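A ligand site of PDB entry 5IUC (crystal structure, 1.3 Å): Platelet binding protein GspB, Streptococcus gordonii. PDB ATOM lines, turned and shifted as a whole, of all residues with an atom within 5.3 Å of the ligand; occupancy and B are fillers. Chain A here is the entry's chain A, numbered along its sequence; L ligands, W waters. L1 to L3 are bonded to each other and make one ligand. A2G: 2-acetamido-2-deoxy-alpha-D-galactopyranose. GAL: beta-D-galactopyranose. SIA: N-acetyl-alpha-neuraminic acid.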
ATOM      1  N   TRP A  47       9.104  17.342 -17.233  1.00  0.00           N
ATOM      2  CA  TRP A  47       8.294  16.144 -17.154  1.00  0.00           C
ATOM      3  C   TRP A  47       7.175  16.118 -18.168  1.00  0.00           C
ATOM      4  O   TRP A  47       7.015  17.059 -18.985  1.00  0.00           O
ATOM      5  CB  TRP A  47       7.784  15.912 -15.748  1.00  0.00           C
ATOM      6  CG  TRP A  47       6.643  16.785 -15.265  1.00  0.00           C
ATOM      7  CD1 TRP A  47       6.235  17.976 -15.770  1.00  0.00           C
ATOM      8  CD2 TRP A  47       5.754  16.478 -14.188  1.00  0.00           C
ATOM      9  NE1 TRP A  47       5.182  18.459 -15.053  1.00  0.00           N
ATOM     10  CE2 TRP A  47       4.854  17.542 -14.084  1.00  0.00           C
ATOM     11  CE3 TRP A  47       5.653  15.410 -13.288  1.00  0.00           C
ATOM     12  CZ2 TRP A  47       3.866  17.603 -13.101  1.00  0.00           C
ATOM     13  CZ3 TRP A  47       4.642  15.446 -12.334  1.00  0.00           C
ATOM     14  CH2 TRP A  47       3.776  16.540 -12.250  1.00  0.00           C
ATOM     15  N   LEU A  48       6.395  15.054 -18.139  1.00  0.00           N
ATOM     16  CA  LEU A  48       5.346  14.862 -19.135  1.00  0.00           C
ATOM     17  C   LEU A  48       4.272  15.941 -19.161  1.00  0.00           C
ATOM     18  O   LEU A  48       3.866  16.377 -20.223  1.00  0.00           O
ATOM     19  CB  LEU A  48       4.648  13.510 -18.894  1.00  0.00           C
ATOM     20  CG  LEU A  48       3.432  13.185 -19.777  1.00  0.00           C
ATOM     21  CD1 LEU A  48       3.819  13.020 -21.244  1.00  0.00           C
ATOM     22  CD2 LEU A  48       2.746  11.942 -19.242  1.00  0.00           C
ATOM     23  N   TYR A  49       3.776  16.333 -17.991  1.00  0.00           N
ATOM     24  CA  TYR A  49       2.460  16.985 -17.933  1.00  0.00           C
ATOM     25  C   TYR A  49       2.471  18.452 -18.262  1.00  0.00           C
ATOM     26  O   TYR A  49       1.418  19.004 -18.661  1.00  0.00           O
ATOM     27  CB  TYR A  49       1.853  16.798 -16.543  1.00  0.00           C
ATOM     28  CG  TYR A  49       1.726  15.380 -16.141  1.00  0.00           C
ATOM     29  CD1 TYR A  49       0.695  14.595 -16.611  1.00  0.00           C
ATOM     30  CD2 TYR A  49       2.665  14.831 -15.313  1.00  0.00           C
ATOM     31  CE1 TYR A  49       0.614  13.258 -16.241  1.00  0.00           C
ATOM     32  CE2 TYR A  49       2.607  13.516 -14.947  1.00  0.00           C
ATOM     33  CZ  TYR A  49       1.555  12.728 -15.391  1.00  0.00           C
ATOM     34  OH  TYR A  49       1.437  11.395 -15.050  1.00  0.00           O
ATOM     35  N   GLY A  54       8.961  18.923 -12.690  1.00  0.00           N
ATOM     36  CA  GLY A  54       8.133  17.812 -12.245  1.00  0.00           C
ATOM     37  C   GLY A  54       8.090  17.616 -10.752  1.00  0.00           C
ATOM     38  O   GLY A  54       9.028  17.900  -9.997  1.00  0.00           O
ATOM     39  N   ARG A  55       6.937  17.125 -10.289  1.00  0.00           N
ATOM     40  CA  ARG A  55       6.759  16.777  -8.894  1.00  0.00           C
ATOM     41  C   ARG A  55       7.767  15.776  -8.421  1.00  0.00           C
ATOM     42  O   ARG A  55       7.976  14.727  -9.037  1.00  0.00           O
ATOM     43  CB  ARG A  55       5.362  16.199  -8.650  1.00  0.00           C
ATOM     44  CG  ARG A  55       5.146  15.882  -7.146  1.00  0.00           C
ATOM     45  CD  ARG A  55       4.091  14.822  -6.818  1.00  0.00           C
ATOM     46  NE  ARG A  55       4.439  13.445  -7.192  1.00  0.00           N
ATOM     47  CZ  ARG A  55       4.048  12.828  -8.315  1.00  0.00           C
ATOM     48  NH1 ARG A  55       3.320  13.442  -9.233  1.00  0.00           N
ATOM     49  NH2 ARG A  55       4.406  11.574  -8.519  1.00  0.00           N
ATOM     50  N   GLY A  56       8.378  16.050  -7.297  1.00  0.00           N
ATOM     51  CA  GLY A  56       9.392  15.143  -6.770  1.00  0.00           C
ATOM     52  C   GLY A  56      10.779  15.462  -7.303  1.00  0.00           C
ATOM     53  O   GLY A  56      11.771  14.978  -6.745  1.00  0.00           O
ATOM     54  N   THR A  57      10.855  16.270  -8.361  1.00  0.00           N
ATOM     55  CA  THR A  57      12.138  16.649  -8.972  1.00  0.00           C
ATOM     56  C   THR A  57      12.164  18.147  -9.264  1.00  0.00           C
ATOM     57  O   THR A  57      12.658  18.595 -10.300  1.00  0.00           O
ATOM     58  CB  THR A  57      12.448  15.851 -10.249  1.00  0.00           C
ATOM     59  OG1 THR A  57      11.457  16.099 -11.245  1.00  0.00           O
ATOM     60  CG2 THR A  57      12.482  14.381  -9.961  1.00  0.00           C
ATOM     61  N   THR A  84      12.542  11.064  -2.640  1.00  0.00           N
ATOM     62  CA  THR A  84      12.182   9.661  -2.793  1.00  0.00           C
ATOM     63  C   THR A  84      13.061   8.982  -3.837  1.00  0.00           C
ATOM     64  O   THR A  84      13.184   9.470  -4.961  1.00  0.00           O
ATOM     65  CB  THR A  84      10.707   9.554  -3.183  1.00  0.00           C
ATOM     66  OG1 THR A  84       9.912  10.186  -2.167  1.00  0.00           O
ATOM     67  CG2 THR A  84      10.263   8.094  -3.392  1.00  0.00           C
ATOM     68  N   ILE A  85      13.715   7.884  -3.484  1.00  0.00           N
ATOM     69  CA  ILE A  85      14.545   7.219  -4.466  1.00  0.00           C
ATOM     70  C   ILE A  85      13.721   6.490  -5.513  1.00  0.00           C
ATOM     71  O   ILE A  85      12.557   6.131  -5.275  1.00  0.00           O
ATOM     72  CB  ILE A  85      15.514   6.227  -3.815  1.00  0.00           C
ATOM     73  CG1 ILE A  85      14.762   5.088  -3.129  1.00  0.00           C
ATOM     74  CG2 ILE A  85      16.415   6.954  -2.824  1.00  0.00           C
ATOM     75  CD1 ILE A  85      15.731   3.995  -2.655  1.00  0.00           C
ATOM     76  N   GLY A  86      14.310   6.230  -6.658  1.00  0.00           N
ATOM     77  CA  GLY A  86      13.596   5.574  -7.733  1.00  0.00           C
ATOM     78  C   GLY A  86      13.853   6.250  -9.075  1.00  0.00           C
ATOM     79  O   GLY A  86      14.810   7.056  -9.226  1.00  0.00           O
ATOM     80  N   ASP A  87      12.969   5.971 -10.013  1.00  0.00           N
ATOM     81  CA  ASP A  87      13.132   6.375 -11.395  1.00  0.00           C
ATOM     82  C   ASP A  87      12.161   7.463 -11.757  1.00  0.00           C
ATOM     83  O   ASP A  87      11.002   7.431 -11.328  1.00  0.00           O
ATOM     84  CB  ASP A  87      12.846   5.186 -12.321  1.00  0.00           C
ATOM     85  CG  ASP A  87      13.857   4.059 -12.181  1.00  0.00           C
ATOM     86  OD1 ASP A  87      14.939   4.280 -11.628  1.00  0.00           O
ATOM     87  OD2 ASP A  87      13.538   2.940 -12.644  1.00  0.00           O
ATOM     88  N   TYR A  88      12.598   8.431 -12.553  1.00  0.00           N
ATOM     89  CA  TYR A  88      11.757   9.539 -12.977  1.00  0.00           C
ATOM     90  C   TYR A  88      11.967   9.770 -14.471  1.00  0.00           C
ATOM     91  O   TYR A  88      13.071  10.178 -14.891  1.00  0.00           O
ATOM     92  CB  TYR A  88      12.125  10.778 -12.191  1.00  0.00           C
ATOM     93  CG  TYR A  88      11.900  10.656 -10.709  1.00  0.00           C
ATOM     94  CD1 TYR A  88      12.842  10.028  -9.880  1.00  0.00           C
ATOM     95  CD2 TYR A  88      10.718  11.113 -10.138  1.00  0.00           C
ATOM     96  CE1 TYR A  88      12.614   9.919  -8.520  1.00  0.00           C
ATOM     97  CE2 TYR A  88      10.504  11.004  -8.775  1.00  0.00           C
ATOM     98  CZ  TYR A  88      11.449  10.388  -7.985  1.00  0.00           C
ATOM     99  OH  TYR A  88      11.175  10.321  -6.611  1.00  0.00           O
ATOM    100  N   THR A  89      10.973   9.522 -15.296  1.00  0.00           N
ATOM    101  CA  THR A  89      11.090   9.782 -16.724  1.00  0.00           C
ATOM    102  C   THR A  89      10.977  11.273 -17.007  1.00  0.00           C
ATOM    103  O   THR A  89      10.012  11.933 -16.601  1.00  0.00           O
ATOM    104  CB  THR A  89      10.023   9.044 -17.486  1.00  0.00           C
ATOM    105  OG1 THR A  89      10.085   7.657 -17.183  1.00  0.00           O
ATOM    106  CG2 THR A  89      10.194   9.253 -18.970  1.00  0.00           C
ATOM    107  N   ARG A  90      11.970  11.827 -17.693  1.00  0.00           N
ATOM    108  CA  ARG A  90      11.990  13.232 -18.038  1.00  0.00           C
ATOM    109  C   ARG A  90      12.402  13.365 -19.508  1.00  0.00           C
ATOM    110  O   ARG A  90      12.728  12.382 -20.153  1.00  0.00           O
ATOM    111  CB  ARG A  90      12.902  14.021 -17.089  1.00  0.00           C
ATOM    112  CG  ARG A  90      12.477  13.972 -15.612  1.00  0.00           C
ATOM    113  CD  ARG A  90      11.181  14.677 -15.337  1.00  0.00           C
ATOM    114  NE  ARG A  90      10.750  14.728 -13.923  1.00  0.00           N
ATOM    115  CZ  ARG A  90       9.914  13.886 -13.336  1.00  0.00           C
ATOM    116  NH1 ARG A  90       9.411  12.838 -13.976  1.00  0.00           N
ATOM    117  NH2 ARG A  90       9.554  14.153 -12.078  1.00  0.00           N
ATOM    118  N   TYR A  91      12.364  14.603 -20.008  1.00  0.00           N
ATOM    119  CA  TYR A  91      12.474  14.856 -21.439  1.00  0.00           C
ATOM    120  C   TYR A  91      13.318  16.082 -21.703  1.00  0.00           C
ATOM    121  O   TYR A  91      13.072  17.135 -21.115  1.00  0.00           O
ATOM    122  CB  TYR A  91      11.078  15.092 -22.042  1.00  0.00           C
ATOM    123  CG  TYR A  91      10.125  13.955 -21.792  1.00  0.00           C
ATOM    124  CD1 TYR A  91       9.348  13.912 -20.661  1.00  0.00           C
ATOM    125  CD2 TYR A  91      10.005  12.912 -22.697  1.00  0.00           C
ATOM    126  CE1 TYR A  91       8.471  12.860 -20.416  1.00  0.00           C
ATOM    127  CE2 TYR A  91       9.140  11.844 -22.440  1.00  0.00           C
ATOM    128  CZ  TYR A  91       8.368  11.835 -21.294  1.00  0.00           C
ATOM    129  OH  TYR A  91       7.498  10.822 -21.012  1.00  0.00           O
ATOM    130  N   GLY A 109       3.115  11.375 -24.468  1.00  0.00           N
ATOM    131  CA  GLY A 109       2.052  10.663 -23.752  1.00  0.00           C
ATOM    132  C   GLY A 109       1.707   9.347 -24.428  1.00  0.00           C
ATOM    133  O   GLY A 109       1.504   8.326 -23.751  1.00  0.00           O
ATOM    134  N   ASN A 110       1.669   9.389 -25.740  1.00  0.00           N
ATOM    135  CA  ASN A 110       1.409   8.163 -26.459  1.00  0.00           C
ATOM    136  C   ASN A 110       2.497   7.128 -26.260  1.00  0.00           C
ATOM    137  O   ASN A 110       2.216   5.954 -26.113  1.00  0.00           O
ATOM    138  CB  ASN A 110       1.147   8.435 -27.909  1.00  0.00           C
ATOM    139  CG  ASN A 110      -0.259   8.962 -28.121  1.00  0.00           C
ATOM    140  OD1 ASN A 110      -1.206   8.518 -27.463  1.00  0.00           O
ATOM    141  ND2 ASN A 110      -0.399   9.915 -28.994  1.00  0.00           N
ATOM    142  N   ALA A 112       4.267   6.911 -23.584  1.00  0.00           N
ATOM    143  CA  ALA A 112       4.131   6.437 -22.204  1.00  0.00           C
ATOM    144  C   ALA A 112       3.079   5.330 -22.096  1.00  0.00           C
ATOM    145  O   ALA A 112       3.317   4.274 -21.522  1.00  0.00           O
ATOM    146  CB  ALA A 112       3.788   7.582 -21.287  1.00  0.00           C
ATOM    147  N   VAL A 113       1.937   5.526 -22.740  1.00  0.00           N
ATOM    148  CA  VAL A 113       0.891   4.486 -22.716  1.00  0.00           C
ATOM    149  C   VAL A 113       1.424   3.181 -23.299  1.00  0.00           C
ATOM    150  O   VAL A 113       1.134   2.088 -22.794  1.00  0.00           O
ATOM    151  CB  VAL A 113      -0.332   4.893 -23.519  1.00  0.00           C
ATOM    152  CG1 VAL A 113      -1.354   3.745 -23.554  1.00  0.00           C
ATOM    153  CG2 VAL A 113      -0.960   6.146 -22.974  1.00  0.00           C
HETATM  154  O5  A2G L   1      -1.257   8.815 -18.787  1.00  0.00           O
HETATM  155  C1  A2G L   1      -1.409   9.096 -17.420  1.00  0.00           C
HETATM  156  O1  A2G L   1      -1.398  10.511 -17.291  1.00  0.00           O
HETATM  157  C2  A2G L   1      -0.297   8.447 -16.606  1.00  0.00           C
HETATM  158  N2  A2G L   1      -0.259   8.934 -15.246  1.00  0.00           N
HETATM  159  C3  A2G L   1       1.060   8.846 -17.157  1.00  0.00           C
HETATM  160  O3  A2G L   1       2.034   8.070 -16.461  1.00  0.00           O
HETATM  161  C4  A2G L   1       1.139   8.580 -18.653  1.00  0.00           C
HETATM  162  O4  A2G L   1       1.070   7.166 -18.918  1.00  0.00           O
HETATM  163  C5  A2G L   1      -0.012   9.273 -19.347  1.00  0.00           C
HETATM  164  C6  A2G L   1      -0.094   8.969 -20.810  1.00  0.00           C
HETATM  165  O6  A2G L   1      -1.057   9.845 -21.441  1.00  0.00           O
HETATM  166  C7  A2G L   1      -0.167   8.163 -14.157  1.00  0.00           C
HETATM  167  O7  A2G L   1      -0.172   6.949 -14.251  1.00  0.00           O
HETATM  168  C8  A2G L   1      -0.030   8.851 -12.824  1.00  0.00           C
HETATM  169  C1  GAL L   2       3.307   8.576 -16.246  1.00  0.00           C
HETATM  170  C2  GAL L   2       3.916   7.697 -15.188  1.00  0.00           C
HETATM  171  C3  GAL L   2       5.427   7.893 -15.079  1.00  0.00           C
HETATM  172  C4  GAL L   2       6.068   7.918 -16.489  1.00  0.00           C
HETATM  173  C5  GAL L   2       5.326   8.957 -17.311  1.00  0.00           C
HETATM  174  C6  GAL L   2       5.816   9.200 -18.690  1.00  0.00           C
HETATM  175  O2  GAL L   2       3.357   8.009 -13.938  1.00  0.00           O
HETATM  176  O3  GAL L   2       5.947   6.792 -14.312  1.00  0.00           O
HETATM  177  O4  GAL L   2       5.955   6.649 -17.088  1.00  0.00           O
HETATM  178  O5  GAL L   2       3.962   8.495 -17.469  1.00  0.00           O
HETATM  179  O6  GAL L   2       6.975  10.045 -18.566  1.00  0.00           O
HETATM  180  C1  SIA L   3       8.252   7.561 -14.303  1.00  0.00           C
HETATM  181  C2  SIA L   3       6.997   7.055 -13.443  1.00  0.00           C
HETATM  182  C3  SIA L   3       7.242   5.749 -12.668  1.00  0.00           C
HETATM  183  C4  SIA L   3       8.230   5.898 -11.536  1.00  0.00           C
HETATM  184  C5  SIA L   3       7.793   7.036 -10.620  1.00  0.00           C
HETATM  185  C6  SIA L   3       7.627   8.310 -11.495  1.00  0.00           C
HETATM  186  C7  SIA L   3       7.179   9.560 -10.745  1.00  0.00           C
HETATM  187  C8  SIA L   3       6.751  10.644 -11.739  1.00  0.00           C
HETATM  188  C9  SIA L   3       6.545  11.988 -11.090  1.00  0.00           C
HETATM  189  C10 SIA L   3       8.617   7.121  -8.275  1.00  0.00           C
HETATM  190  C11 SIA L   3       9.822   7.353  -7.394  1.00  0.00           C
HETATM  191  N5  SIA L   3       8.803   7.248  -9.610  1.00  0.00           N
HETATM  192  O1A SIA L   3       8.423   8.812 -14.302  1.00  0.00           O
HETATM  193  O1B SIA L   3       8.907   6.700 -14.913  1.00  0.00           O
HETATM  194  O4  SIA L   3       8.326   4.685 -10.763  1.00  0.00           O
HETATM  195  O6  SIA L   3       6.631   8.045 -12.476  1.00  0.00           O
HETATM  196  O7  SIA L   3       6.052   9.254  -9.905  1.00  0.00           O
HETATM  197  O8  SIA L   3       7.749  10.854 -12.731  1.00  0.00           O
HETATM  198  O9  SIA L   3       7.755  12.483 -10.519  1.00  0.00           O
HETATM  199  O10 SIA L   3       7.528   6.804  -7.779  1.00  0.00           O
HETATM  200  O   HOH W   1       1.400   5.163 -15.821  1.00  0.00           O
HETATM  201  O   HOH W   2       5.955   3.901  -9.439  1.00  0.00           O
HETATM  202  O   HOH W   3       8.100   6.137 -18.637  1.00  0.00           O
HETATM  203  O   HOH W   4       3.870   7.773 -10.616  1.00  0.00           O
HETATM  204  O   HOH W   5       4.887   6.180  -8.114  1.00  0.00           O
HETATM  205  O   HOH W   6       3.489  10.622 -13.454  1.00  0.00           O
HETATM  206  O   HOH W   7       6.162  10.382  -7.355  1.00  0.00           O
HETATM  207  O   HOH W   8       7.480   6.287  -5.148  1.00  0.00           O
HETATM  208  O   HOH W   9       3.269   5.920 -12.191  1.00  0.00           O
HETATM  209  O   HOH W  10      10.653   4.155  -9.193  1.00  0.00           O
HETATM  210  O   HOH W  11       7.243  12.485 -16.938  1.00  0.00           O
HETATM  211  O   HOH W  12      -1.425   5.715 -19.117  1.00  0.00           O
HETATM  212  O   HOH W  13       5.803  11.739 -14.631  1.00  0.00           O
HETATM  213  O   HOH W  14       9.269   4.117 -15.201  1.00  0.00           O
HETATM  214  O   HOH W  15       3.256   5.676 -18.042  1.00  0.00           O
HETATM  215  O   HOH W  16       9.405   2.636 -12.234  1.00  0.00           O
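O of Asp 87 sits at hydrogen-bond distance from N5 of SIA L3, 2.8 Å away. N of Thr 89 is in hydrogen-bond range of O1A of SIA L3 (2.8 Å). NH1 of Arg 90 sits at hydrogen-bond distance from O8 of SIA L3 (2.9 Å). The side-chain hydroxyl (OG1) of Thr 89 lies within hydrogen-bond range of an oxygen (O1B) of SIA L3 (2.7 Å). An oxygen (O6) of GAL L2 lies within hydrogen-bond range of the side-chain hydroxyl of Tyr 91 (2.6 Å). The backbone carbonyl oxygen (O) of Arg 55 is in hydrogen-bond range of an oxygen (O9) of SIA L3, at 2.7 Å. O7 of SIA L3 sits at hydrogen-bond distance from NH2 of Arg 55, 3.2 Å away. N2 of A2G L1 is in hydrogen-bond range of OH of Tyr 49 (3.0 Å).
The side-chain hydroxyl of Thr 57 sits at hydrogen-bond distance from the guanidinium group of Arg 90, at 2.8 Å. The side-chain hydroxyl of Tyr 88 lies within hydrogen-bond range of the backbone carbonyl oxygen of Thr 84 (2.7 Å). O of Arg 55 is in hydrogen-bond range of NH2 of Arg 90 (3.5 Å).
CD2 of Leu 48 touches C4 of A2G L1, at 3.8 Å. Ile 85 touches the ligand. Tyr 88 touches the ligand. O of Gly 109 touches C6 of A2G L1, at 3.4 Å. CB of Ala 112 touches O4 of A2G L1, 3.6 Å away. CG2 of Val 113 touches C6 of A2G L1, 3.7 Å away. Hydrophobic or aromatic side chains that line the ligand: Leu 48, Tyr 49, Tyr 88, Tyr 91, Ala 112 and Val 113. Along chain A the residues within 4 Å of the ligand span positions 48 to 113. The nearest printed residue that does not touch the ligand is Thr 84 (4.1 Å).
Water W6 bridges O2 of GAL L2 and OH of Tyr 49. Water W3 lies within hydrogen-bond range of an oxygen (O4) of GAL L2 and the side-chain hydroxyl of Thr 89. Water W7 bridges the guanidinium group (NH2) of Arg 55 (2.4 Å) and an oxygen (O7) of SIA L3 (2.8 Å). Water W10 bridges O4 of SIA L3 (2.9 Å) and N of Asp 87 (3.1 Å). Water W11 lies within hydrogen-bond range of the backbone carbonyl oxygen (O) of Thr 89, an oxygen (O6) of GAL L2 and the backbone NH (N) of Leu 48.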
